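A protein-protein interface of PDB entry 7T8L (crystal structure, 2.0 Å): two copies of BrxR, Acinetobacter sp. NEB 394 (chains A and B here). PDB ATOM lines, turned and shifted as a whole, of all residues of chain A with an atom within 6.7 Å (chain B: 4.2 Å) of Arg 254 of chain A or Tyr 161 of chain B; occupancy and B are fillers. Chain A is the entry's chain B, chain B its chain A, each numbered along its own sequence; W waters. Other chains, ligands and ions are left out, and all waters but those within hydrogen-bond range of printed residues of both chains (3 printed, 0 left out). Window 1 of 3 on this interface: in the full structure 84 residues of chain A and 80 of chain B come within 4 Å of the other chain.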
ATOM      1  N   ILE A  84       7.810  11.210 -29.671  1.00  0.00           N
ATOM      2  CA  ILE A  84       8.882  11.368 -30.705  1.00  0.00           C
ATOM      3  C   ILE A  84      10.140  11.976 -30.063  1.00  0.00           C
ATOM      4  O   ILE A  84      11.216  11.702 -30.562  1.00  0.00           O
ATOM      5  CB  ILE A  84       8.425  12.142 -31.952  1.00  0.00           C
ATOM      6  CG1 ILE A  84       9.470  12.025 -33.055  1.00  0.00           C
ATOM      7  CG2 ILE A  84       8.077  13.593 -31.650  1.00  0.00           C
ATOM      8  CD1 ILE A  84       9.021  12.582 -34.361  1.00  0.00           C
ATOM      9  N   ASN A  85      10.036  12.714 -28.964  1.00  0.00           N
ATOM     10  CA  ASN A  85      11.234  13.194 -28.218  1.00  0.00           C
ATOM     11  C   ASN A  85      12.253  12.056 -28.006  1.00  0.00           C
ATOM     12  O   ASN A  85      13.457  12.335 -28.090  1.00  0.00           O
ATOM     13  CB  ASN A  85      10.902  13.753 -26.839  1.00  0.00           C
ATOM     14  CG  ASN A  85       9.784  14.766 -26.870  1.00  0.00           C
ATOM     15  OD1 ASN A  85       8.701  14.489 -27.399  1.00  0.00           O
ATOM     16  ND2 ASN A  85      10.043  15.928 -26.282  1.00  0.00           N
ATOM     17  N   LEU A  88      14.361  11.538 -31.266  1.00  0.00           N
ATOM     18  CA  LEU A  88      15.328  12.642 -31.423  1.00  0.00           C
ATOM     19  C   LEU A  88      16.474  12.485 -30.394  1.00  0.00           C
ATOM     20  O   LEU A  88      17.662  12.672 -30.782  1.00  0.00           O
ATOM     21  CB  LEU A  88      14.631  14.002 -31.297  1.00  0.00           C
ATOM     22  CG  LEU A  88      15.592  15.168 -31.545  1.00  0.00           C
ATOM     23  CD1 LEU A  88      16.297  15.018 -32.891  1.00  0.00           C
ATOM     24  CD2 LEU A  88      14.889  16.502 -31.441  1.00  0.00           C
ATOM     25  N   LEU A 109      16.889  15.114 -41.360  1.00  0.00           N
ATOM     26  CA  LEU A 109      16.395  15.623 -40.052  1.00  0.00           C
ATOM     27  C   LEU A 109      17.192  16.863 -39.611  1.00  0.00           C
ATOM     28  O   LEU A 109      18.430  16.779 -39.570  1.00  0.00           O
ATOM     29  CB  LEU A 109      16.429  14.487 -39.025  1.00  0.00           C
ATOM     30  CG  LEU A 109      16.060  14.879 -37.593  1.00  0.00           C
ATOM     31  CD1 LEU A 109      14.616  15.263 -37.476  1.00  0.00           C
ATOM     32  CD2 LEU A 109      16.365  13.747 -36.617  1.00  0.00           C
ATOM     33  N   ALA A 110      16.497  17.972 -39.321  1.00  0.00           N
ATOM     34  CA  ALA A 110      17.073  19.225 -38.801  1.00  0.00           C
ATOM     35  C   ALA A 110      16.366  19.563 -37.496  1.00  0.00           C
ATOM     36  O   ALA A 110      15.119  19.419 -37.400  1.00  0.00           O
ATOM     37  CB  ALA A 110      16.953  20.326 -39.813  1.00  0.00           C
ATOM     38  N   ALA A 111      17.137  19.959 -36.509  1.00  0.00           N
ATOM     39  CA  ALA A 111      16.611  20.311 -35.181  1.00  0.00           C
ATOM     40  C   ALA A 111      17.142  21.683 -34.814  1.00  0.00           C
ATOM     41  O   ALA A 111      18.382  21.833 -34.751  1.00  0.00           O
ATOM     42  CB  ALA A 111      16.968  19.253 -34.162  1.00  0.00           C
ATOM     43  N   VAL A 112      16.229  22.615 -34.584  1.00  0.00           N
ATOM     44  CA  VAL A 112      16.530  24.012 -34.202  1.00  0.00           C
ATOM     45  C   VAL A 112      16.952  24.024 -32.732  1.00  0.00           C
ATOM     46  O   VAL A 112      16.143  23.633 -31.891  1.00  0.00           O
ATOM     47  CB  VAL A 112      15.338  24.936 -34.457  1.00  0.00           C
ATOM     48  CG1 VAL A 112      15.629  26.388 -34.044  1.00  0.00           C
ATOM     49  CG2 VAL A 112      14.894  24.863 -35.905  1.00  0.00           C
ATOM     50  N   GLN A 113      18.159  24.510 -32.440  1.00  0.00           N
ATOM     51  CA  GLN A 113      18.743  24.464 -31.071  1.00  0.00           C
ATOM     52  C   GLN A 113      18.962  25.868 -30.545  1.00  0.00           C
ATOM     53  O   GLN A 113      18.938  26.825 -31.346  1.00  0.00           O
ATOM     54  CB  GLN A 113      20.067  23.705 -31.088  1.00  0.00           C
ATOM     55  CG  GLN A 113      19.850  22.233 -31.337  1.00  0.00           C
ATOM     56  CD  GLN A 113      21.100  21.392 -31.296  1.00  0.00           C
ATOM     57  OE1 GLN A 113      21.032  20.202 -31.041  1.00  0.00           O
ATOM     58  NE2 GLN A 113      22.229  21.980 -31.649  1.00  0.00           N
ATOM     59  N   THR A 162      15.258  26.182 -18.243  1.00  0.00           N
ATOM     60  CA  THR A 162      13.859  26.540 -18.617  1.00  0.00           C
ATOM     61  C   THR A 162      13.535  26.150 -20.062  1.00  0.00           C
ATOM     62  O   THR A 162      12.349  26.288 -20.445  1.00  0.00           O
ATOM     63  CB  THR A 162      13.570  28.030 -18.466  1.00  0.00           C
ATOM     64  OG1 THR A 162      14.312  28.698 -19.492  1.00  0.00           O
ATOM     65  CG2 THR A 162      13.929  28.584 -17.106  1.00  0.00           C
ATOM     66  N   GLY A 163      14.520  25.683 -20.817  1.00  0.00           N
ATOM     67  CA  GLY A 163      14.443  25.538 -22.284  1.00  0.00           C
ATOM     68  C   GLY A 163      15.014  26.756 -22.981  1.00  0.00           C
ATOM     69  O   GLY A 163      15.243  26.684 -24.173  1.00  0.00           O
ATOM     70  N   PHE A 164      15.280  27.841 -22.267  1.00  0.00           N
ATOM     71  CA  PHE A 164      15.859  29.079 -22.853  1.00  0.00           C
ATOM     72  C   PHE A 164      17.063  29.570 -22.044  1.00  0.00           C
ATOM     73  O   PHE A 164      18.033  30.123 -22.655  1.00  0.00           O
ATOM     74  CB  PHE A 164      14.813  30.187 -22.928  1.00  0.00           C
ATOM     75  CG  PHE A 164      13.579  29.741 -23.654  1.00  0.00           C
ATOM     76  CD1 PHE A 164      13.528  29.828 -25.038  1.00  0.00           C
ATOM     77  CD2 PHE A 164      12.514  29.178 -22.959  1.00  0.00           C
ATOM     78  CE1 PHE A 164      12.422  29.369 -25.726  1.00  0.00           C
ATOM     79  CE2 PHE A 164      11.416  28.715 -23.650  1.00  0.00           C
ATOM     80  CZ  PHE A 164      11.366  28.840 -25.035  1.00  0.00           C
ATOM     81  N   HIS A 249       5.363  29.656 -14.677  1.00  0.00           N
ATOM     82  CA  HIS A 249       5.633  30.716 -15.688  1.00  0.00           C
ATOM     83  C   HIS A 249       6.528  30.121 -16.773  1.00  0.00           C
ATOM     84  O   HIS A 249       6.258  30.349 -17.939  1.00  0.00           O
ATOM     85  CB  HIS A 249       6.210  31.979 -15.030  1.00  0.00           C
ATOM     86  CG  HIS A 249       5.144  32.824 -14.390  1.00  0.00           C
ATOM     87  ND1 HIS A 249       4.083  33.363 -15.121  1.00  0.00           N
ATOM     88  CD2 HIS A 249       4.936  33.201 -13.102  1.00  0.00           C
ATOM     89  CE1 HIS A 249       3.292  34.041 -14.307  1.00  0.00           C
ATOM     90  NE2 HIS A 249       3.790  33.963 -13.071  1.00  0.00           N
ATOM     91  N   TYR A 250       7.524  29.324 -16.398  1.00  0.00           N
ATOM     92  CA  TYR A 250       8.494  28.750 -17.373  1.00  0.00           C
ATOM     93  C   TYR A 250       7.794  27.692 -18.225  1.00  0.00           C
ATOM     94  O   TYR A 250       8.044  27.682 -19.437  1.00  0.00           O
ATOM     95  CB  TYR A 250       9.746  28.233 -16.680  1.00  0.00           C
ATOM     96  CG  TYR A 250      10.441  29.295 -15.867  1.00  0.00           C
ATOM     97  CD1 TYR A 250      10.961  30.435 -16.465  1.00  0.00           C
ATOM     98  CD2 TYR A 250      10.599  29.148 -14.504  1.00  0.00           C
ATOM     99  CE1 TYR A 250      11.644  31.394 -15.738  1.00  0.00           C
ATOM    100  CE2 TYR A 250      11.211  30.132 -13.741  1.00  0.00           C
ATOM    101  CZ  TYR A 250      11.738  31.249 -14.365  1.00  0.00           C
ATOM    102  OH  TYR A 250      12.351  32.191 -13.618  1.00  0.00           O
ATOM    103  N   THR A 251       6.914  26.863 -17.641  1.00  0.00           N
ATOM    104  CA  THR A 251       6.153  25.857 -18.395  1.00  0.00           C
ATOM    105  C   THR A 251       5.307  26.551 -19.454  1.00  0.00           C
ATOM    106  O   THR A 251       5.308  26.098 -20.604  1.00  0.00           O
ATOM    107  CB  THR A 251       5.320  24.962 -17.472  1.00  0.00           C
ATOM    108  OG1 THR A 251       6.312  24.362 -16.639  1.00  0.00           O
ATOM    109  CG2 THR A 251       4.495  23.959 -18.256  1.00  0.00           C
ATOM    110  N   LEU A 252       4.593  27.597 -19.076  1.00  0.00           N
ATOM    111  CA  LEU A 252       3.716  28.346 -20.006  1.00  0.00           C
ATOM    112  C   LEU A 252       4.544  28.940 -21.162  1.00  0.00           C
ATOM    113  O   LEU A 252       4.082  28.893 -22.288  1.00  0.00           O
ATOM    114  CB  LEU A 252       3.026  29.457 -19.224  1.00  0.00           C
ATOM    115  CG  LEU A 252       2.039  28.986 -18.154  1.00  0.00           C
ATOM    116  CD1 LEU A 252       1.732  30.133 -17.191  1.00  0.00           C
ATOM    117  CD2 LEU A 252       0.765  28.468 -18.795  1.00  0.00           C
ATOM    118  N   GLN A 253       5.726  29.472 -20.888  1.00  0.00           N
ATOM    119  CA  GLN A 253       6.574  30.056 -21.958  1.00  0.00           C
ATOM    120  C   GLN A 253       7.083  28.913 -22.841  1.00  0.00           C
ATOM    121  O   GLN A 253       7.208  29.115 -24.045  1.00  0.00           O
ATOM    122  CB  GLN A 253       7.707  30.889 -21.365  1.00  0.00           C
ATOM    123  CG  GLN A 253       7.219  32.116 -20.604  1.00  0.00           C
ATOM    124  CD  GLN A 253       8.338  32.823 -19.866  1.00  0.00           C
ATOM    125  OE1 GLN A 253       9.483  32.823 -20.317  1.00  0.00           O
ATOM    126  NE2 GLN A 253       8.018  33.405 -18.711  1.00  0.00           N
ATOM    127  N   ARG A 254       7.326  27.738 -22.260  1.00  0.00           N
ATOM    128  CA  ARG A 254       7.871  26.582 -23.020  1.00  0.00           C
ATOM    129  C   ARG A 254       6.814  26.143 -24.034  1.00  0.00           C
ATOM    130  O   ARG A 254       7.224  25.757 -25.160  1.00  0.00           O
ATOM    131  CB  ARG A 254       8.350  25.486 -22.063  1.00  0.00           C
ATOM    132  CG  ARG A 254       8.926  24.252 -22.744  1.00  0.00           C
ATOM    133  CD  ARG A 254      10.316  24.532 -23.234  1.00  0.00           C
ATOM    134  NE  ARG A 254      10.894  23.485 -24.094  1.00  0.00           N
ATOM    135  CZ  ARG A 254      10.685  23.382 -25.389  1.00  0.00           C
ATOM    136  NH1 ARG A 254       9.806  24.179 -25.994  1.00  0.00           N
ATOM    137  NH2 ARG A 254      11.355  22.476 -26.079  1.00  0.00           N
ATOM    138  N   TYR A 255       5.526  26.235 -23.679  1.00  0.00           N
ATOM    139  CA  TYR A 255       4.376  25.877 -24.548  1.00  0.00           C
ATOM    140  C   TYR A 255       3.954  27.061 -25.447  1.00  0.00           C
ATOM    141  O   TYR A 255       3.038  26.908 -26.303  1.00  0.00           O
ATOM    142  CB  TYR A 255       3.217  25.351 -23.692  1.00  0.00           C
ATOM    143  CG  TYR A 255       3.309  23.889 -23.313  1.00  0.00           C
ATOM    144  CD1 TYR A 255       4.045  23.474 -22.216  1.00  0.00           C
ATOM    145  CD2 TYR A 255       2.640  22.913 -24.041  1.00  0.00           C
ATOM    146  CE1 TYR A 255       4.137  22.139 -21.859  1.00  0.00           C
ATOM    147  CE2 TYR A 255       2.738  21.566 -23.716  1.00  0.00           C
ATOM    148  CZ  TYR A 255       3.478  21.175 -22.610  1.00  0.00           C
ATOM    149  OH  TYR A 255       3.628  19.857 -22.285  1.00  0.00           O
ATOM    150  N   GLN A 256       4.591  28.216 -25.283  1.00  0.00           N
ATOM    151  CA  GLN A 256       4.299  29.459 -26.061  1.00  0.00           C
ATOM    152  C   GLN A 256       2.817  29.862 -25.849  1.00  0.00           C
ATOM    153  O   GLN A 256       2.163  30.299 -26.816  1.00  0.00           O
ATOM    154  CB  GLN A 256       4.611  29.280 -27.544  1.00  0.00           C
ATOM    155  CG  GLN A 256       6.022  28.828 -27.880  1.00  0.00           C
ATOM    156  CD  GLN A 256       6.140  28.585 -29.362  1.00  0.00           C
ATOM    157  OE1 GLN A 256       5.440  27.736 -29.948  1.00  0.00           O
ATOM    158  NE2 GLN A 256       7.040  29.332 -29.981  1.00  0.00           N
ATOM    159  N   THR A 257       2.313  29.735 -24.620  1.00  0.00           N
ATOM    160  CA  THR A 257       0.900  29.969 -24.235  1.00  0.00           C
ATOM    161  C   THR A 257       0.692  31.487 -24.151  1.00  0.00           C
ATOM    162  O   THR A 257       1.646  32.203 -23.706  1.00  0.00           O
ATOM    163  CB  THR A 257       0.608  29.292 -22.882  1.00  0.00           C
ATOM    164  OG1 THR A 257       1.042  27.931 -22.960  1.00  0.00           O
ATOM    165  CG2 THR A 257      -0.844  29.344 -22.463  1.00  0.00           C
ATOM    166  N   VAL B 112      12.857  21.945 -17.684  1.00  0.00           N
ATOM    167  CA  VAL B 112      11.515  22.176 -18.259  1.00  0.00           C
ATOM    168  C   VAL B 112      11.503  21.601 -19.685  1.00  0.00           C
ATOM    169  O   VAL B 112      12.395  21.969 -20.512  1.00  0.00           O
ATOM    170  CB  VAL B 112      11.136  23.662 -18.191  1.00  0.00           C
ATOM    171  CG1 VAL B 112       9.765  23.907 -18.806  1.00  0.00           C
ATOM    172  CG2 VAL B 112      11.155  24.181 -16.770  1.00  0.00           C
ATOM    173  N   GLN B 113      10.576  20.676 -19.957  1.00  0.00           N
ATOM    174  CA  GLN B 113      10.532  19.927 -21.248  1.00  0.00           C
ATOM    175  C   GLN B 113       9.204  20.214 -21.957  1.00  0.00           C
ATOM    176  O   GLN B 113       8.274  20.751 -21.301  1.00  0.00           O
ATOM    177  CB  GLN B 113      10.720  18.437 -20.972  1.00  0.00           C
ATOM    178  CG  GLN B 113      12.043  18.148 -20.294  1.00  0.00           C
ATOM    179  CD  GLN B 113      12.449  16.700 -20.336  1.00  0.00           C
ATOM    180  OE1 GLN B 113      13.595  16.378 -20.620  1.00  0.00           O
ATOM    181  NE2 GLN B 113      11.514  15.814 -20.040  1.00  0.00           N
ATOM    182  N   LEU B 114       9.114  19.878 -23.247  1.00  0.00           N
ATOM    183  CA  LEU B 114       7.834  19.877 -23.998  1.00  0.00           C
ATOM    184  C   LEU B 114       7.629  18.475 -24.560  1.00  0.00           C
ATOM    185  O   LEU B 114       8.084  18.206 -25.663  1.00  0.00           O
ATOM    186  CB  LEU B 114       7.906  20.947 -25.098  1.00  0.00           C
ATOM    187  CG  LEU B 114       6.649  21.144 -25.935  1.00  0.00           C
ATOM    188  CD1 LEU B 114       5.444  21.347 -25.074  1.00  0.00           C
ATOM    189  CD2 LEU B 114       6.778  22.311 -26.876  1.00  0.00           C
ATOM    190  N   VAL B 160      11.734  18.532 -39.704  1.00  0.00           N
ATOM    191  CA  VAL B 160      12.282  19.652 -38.908  1.00  0.00           C
ATOM    192  C   VAL B 160      11.620  19.642 -37.526  1.00  0.00           C
ATOM    193  O   VAL B 160      10.368  19.604 -37.429  1.00  0.00           O
ATOM    194  CB  VAL B 160      12.066  20.995 -39.595  1.00  0.00           C
ATOM    195  CG1 VAL B 160      12.678  22.086 -38.742  1.00  0.00           C
ATOM    196  CG2 VAL B 160      12.605  21.037 -41.018  1.00  0.00           C
ATOM    197  N   TYR B 161      12.434  19.649 -36.483  1.00  0.00           N
ATOM    198  CA  TYR B 161      11.964  19.971 -35.111  1.00  0.00           C
ATOM    199  C   TYR B 161      12.374  21.402 -34.767  1.00  0.00           C
ATOM    200  O   TYR B 161      13.550  21.751 -34.859  1.00  0.00           O
ATOM    201  CB  TYR B 161      12.563  18.995 -34.113  1.00  0.00           C
ATOM    202  CG  TYR B 161      12.219  19.294 -32.684  1.00  0.00           C
ATOM    203  CD1 TYR B 161      10.898  19.303 -32.277  1.00  0.00           C
ATOM    204  CD2 TYR B 161      13.202  19.527 -31.737  1.00  0.00           C
ATOM    205  CE1 TYR B 161      10.560  19.514 -30.945  1.00  0.00           C
ATOM    206  CE2 TYR B 161      12.888  19.721 -30.397  1.00  0.00           C
ATOM    207  CZ  TYR B 161      11.555  19.728 -30.009  1.00  0.00           C
ATOM    208  OH  TYR B 161      11.200  19.957 -28.705  1.00  0.00           O
ATOM    209  N   THR B 162      11.413  22.226 -34.388  1.00  0.00           N
ATOM    210  CA  THR B 162      11.614  23.668 -34.166  1.00  0.00           C
ATOM    211  C   THR B 162      11.973  23.952 -32.712  1.00  0.00           C
ATOM    212  O   THR B 162      12.204  25.103 -32.444  1.00  0.00           O
ATOM    213  CB  THR B 162      10.381  24.478 -34.563  1.00  0.00           C
ATOM    214  OG1 THR B 162       9.363  24.193 -33.597  1.00  0.00           O
ATOM    215  CG2 THR B 162       9.945  24.177 -35.979  1.00  0.00           C
ATOM    216  N   GLY B 163      11.955  22.950 -31.828  1.00  0.00           N
ATOM    217  CA  GLY B 163      11.930  23.171 -30.375  1.00  0.00           C
ATOM    218  C   GLY B 163      10.515  23.254 -29.806  1.00  0.00           C
ATOM    219  O   GLY B 163      10.409  23.222 -28.580  1.00  0.00           O
ATOM    220  N   PHE B 164       9.476  23.381 -30.636  1.00  0.00           N
ATOM    221  CA  PHE B 164       8.044  23.463 -30.192  1.00  0.00           C
ATOM    222  C   PHE B 164       7.155  22.455 -30.926  1.00  0.00           C
ATOM    223  O   PHE B 164       6.180  21.925 -30.345  1.00  0.00           O
ATOM    224  CB  PHE B 164       7.499  24.895 -30.357  1.00  0.00           C
ATOM    225  CG  PHE B 164       8.336  25.939 -29.673  1.00  0.00           C
ATOM    226  CD1 PHE B 164       8.158  26.213 -28.326  1.00  0.00           C
ATOM    227  CD2 PHE B 164       9.330  26.609 -30.363  1.00  0.00           C
ATOM    228  CE1 PHE B 164       8.949  27.143 -27.681  1.00  0.00           C
ATOM    229  CE2 PHE B 164      10.134  27.533 -29.715  1.00  0.00           C
ATOM    230  CZ  PHE B 164       9.919  27.819 -28.377  1.00  0.00           C
ATOM    231  N   ARG B 165       7.475  22.192 -32.184  1.00  0.00           N
ATOM    232  CA  ARG B 165       6.619  21.389 -33.086  1.00  0.00           C
ATOM    233  C   ARG B 165       7.478  20.688 -34.119  1.00  0.00           C
ATOM    234  O   ARG B 165       8.623  21.116 -34.358  1.00  0.00           O
ATOM    235  CB  ARG B 165       5.647  22.276 -33.872  1.00  0.00           C
ATOM    236  CG  ARG B 165       4.538  22.883 -33.030  1.00  0.00           C
ATOM    237  CD  ARG B 165       3.767  23.951 -33.798  1.00  0.00           C
ATOM    238  NE  ARG B 165       2.816  24.645 -32.936  1.00  0.00           N
ATOM    239  CZ  ARG B 165       1.484  24.559 -33.024  1.00  0.00           C
ATOM    240  NH1 ARG B 165       0.912  23.809 -33.951  1.00  0.00           N
ATOM    241  NH2 ARG B 165       0.724  25.238 -32.182  1.00  0.00           N
ATOM    242  N   TRP B 166       6.886  19.700 -34.767  1.00  0.00           N
ATOM    243  CA  TRP B 166       7.508  18.950 -35.881  1.00  0.00           C
ATOM    244  C   TRP B 166       6.785  19.286 -37.184  1.00  0.00           C
ATOM    245  O   TRP B 166       5.509  19.300 -37.222  1.00  0.00           O
ATOM    246  CB  TRP B 166       7.486  17.463 -35.589  1.00  0.00           C
ATOM    247  CG  TRP B 166       8.413  17.018 -34.506  1.00  0.00           C
ATOM    248  CD1 TRP B 166       8.203  17.066 -33.161  1.00  0.00           C
ATOM    249  CD2 TRP B 166       9.682  16.383 -34.690  1.00  0.00           C
ATOM    250  NE1 TRP B 166       9.246  16.494 -32.500  1.00  0.00           N
ATOM    251  CE2 TRP B 166      10.172  16.065 -33.410  1.00  0.00           C
ATOM    252  CE3 TRP B 166      10.432  16.045 -35.814  1.00  0.00           C
ATOM    253  CZ2 TRP B 166      11.420  15.486 -33.217  1.00  0.00           C
ATOM    254  CZ3 TRP B 166      11.648  15.434 -35.633  1.00  0.00           C
ATOM    255  CH2 TRP B 166      12.140  15.166 -34.353  1.00  0.00           C
HETATM  256  O   HOH W   1       9.533  16.347 -29.587  1.00  0.00           O
HETATM  257  O   HOH W   2      13.166  22.232 -23.095  1.00  0.00           O
HETATM  258  O   HOH W   3       4.806  26.968 -32.511  1.00  0.00           O
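Among the printed residues, merely in contact across the chains: Ile 84 of chain A with Trp 166 of chain B (3.2 Å), Leu 88 of chain A with Tyr 161 of chain B (3.5 Å), Leu 109 of chain A with Trp 166 of chain B (3.5 Å), Ala 110 of chain A with Val 160 of chain B (3.2 Å), Ala 111 of chain A with Tyr 161 of chain B (3.4 Å), Val 112 of chain A with Thr 162 of chain B (3.7 Å), Thr 162 of chain A with Val 112 of chain B (3.7 Å), Phe 164 of chain A with Phe 164 of chain B (3.8 Å), Arg 254 of chain A with Val 112 of chain B (3.9 Å), Arg 254 of chain A with Gln 113 of chain B (3.8 Å), Arg 254 of chain A with Leu 114 of chain B (3.7 Å), Arg 254 of chain A with Tyr 161 of chain B (3.6 Å), Arg 254 of chain A with Phe 164 of chain B (3.3 Å), Tyr 255 of chain A with Leu 114 of chain B (3.0 Å) and Gln 256 of chain A with Phe 164 of chain B (3.3 Å).
Val 112 of chain A touches Thr 162 of chain B, and with the chains exchanged Thr 162 of chain A touches Val 112 of chain B.
Phe 164 of chain A touches its own counterpart, Phe 164 of chain B.
The backbone carbonyl oxygen (O) of Leu 114 of chain B is in hydrogen-bond range of the side-chain amide nitrogen (ND2) of Asn 85 of chain A (3.1 Å).
The guanidinium group of Arg 254 of chain A lies within hydrogen-bond range of the backbone carbonyl oxygen of Gly 163 of chain B.
The backbone NH (N) of Val 112 of chain A lies within hydrogen-bond range of the backbone carbonyl oxygen (O) of Tyr 161 of chain B, at 2.8 Å.
The backbone carbonyl oxygen (O) of Ala 110 of chain A sits at hydrogen-bond distance from the backbone NH (N) of Tyr 161 of chain B, at 2.8 Å.
The backbone NH of Phe 164 of chain B is in hydrogen-bond range of the side-chain hydroxyl of Thr 162 of chain B, at 3.1 Å.
OG1 of Thr 162 of chain A lies within hydrogen-bond range of N of Phe 164 of chain A (3.1 Å).
The backbone NH (N) of Arg 165 of chain B sits at hydrogen-bond distance from the side-chain hydroxyl (OG1) of Thr 162 of chain B (3.1 Å).
The side-chain hydroxyl (OH) of Tyr 161 of chain B lies within hydrogen-bond range of the backbone carbonyl oxygen (O) of Gly 163 of chain B.
Of chain B, only Val 112, Gln 113, Leu 114, Tyr 161, Gly 163 and Phe 164 come within 4 Å of Arg 254 of chain A.
Of chain A, only Leu 88 (3.5 Å), Ala 110 (2.8 Å), Ala 111 (3.4 Å), Val 112 (2.8 Å) and Arg 254 (3.6 Å) come within 4 Å of Tyr 161 of chain B.
Of the printed residues of chain B, Val 112 of chain A touches Tyr 161 (2.8 Å) and Thr 162 (3.7 Å).
Printed residues of chain B within 4 Å of Phe 164 of chain A: Phe 164 (3.8 Å).
The nearest residue of chain A that does not touch Tyr 161 of chain B is Asn 85 of chain A (4.8 Å).
Of the 10 printed residues of chain B, 9 touch a printed residue of chain A.
Along chain B the printed residues that touch a printed residue of chain A span positions 112 to 166.
Printed residues of chain A that touch a printed residue of chain B: Ile 84, Asn 85, Leu 88, Leu 109, Ala 110, Ala 111, Val 112, Thr 162, Phe 164, Arg 254, Tyr 255 and Gln 256.
Hydrophobic or aromatic side chains of chain A that line the printed part of chain B: Ile 84, Leu 88, Leu 109, Val 112, Phe 164 and Tyr 255.
Among the printed residues, 19 pairs touch across the chains.
Among the printed residues, no Asp or Glu carboxylate lies within 4 Å of a Lys or Arg side-chain nitrogen of the other chain.
Water W2 lies within hydrogen-bond range of the backbone carbonyl oxygen of Val 112 of chain B (2.7 Å) and the guanidinium group of Arg 254 of chain A (2.8 Å).
Water W3 lies within hydrogen-bond range of the side-chain amide oxygen (OE1) of Gln 256 of chain A (2.7 Å) and the guanidinium group (NE) of Arg 165 of chain B (3.1 Å).
Water W1 lies within hydrogen-bond range of NE1 of Trp 166 of chain B (2.9 Å) and OD1 of Asn 85 of chain A (3.0 Å).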
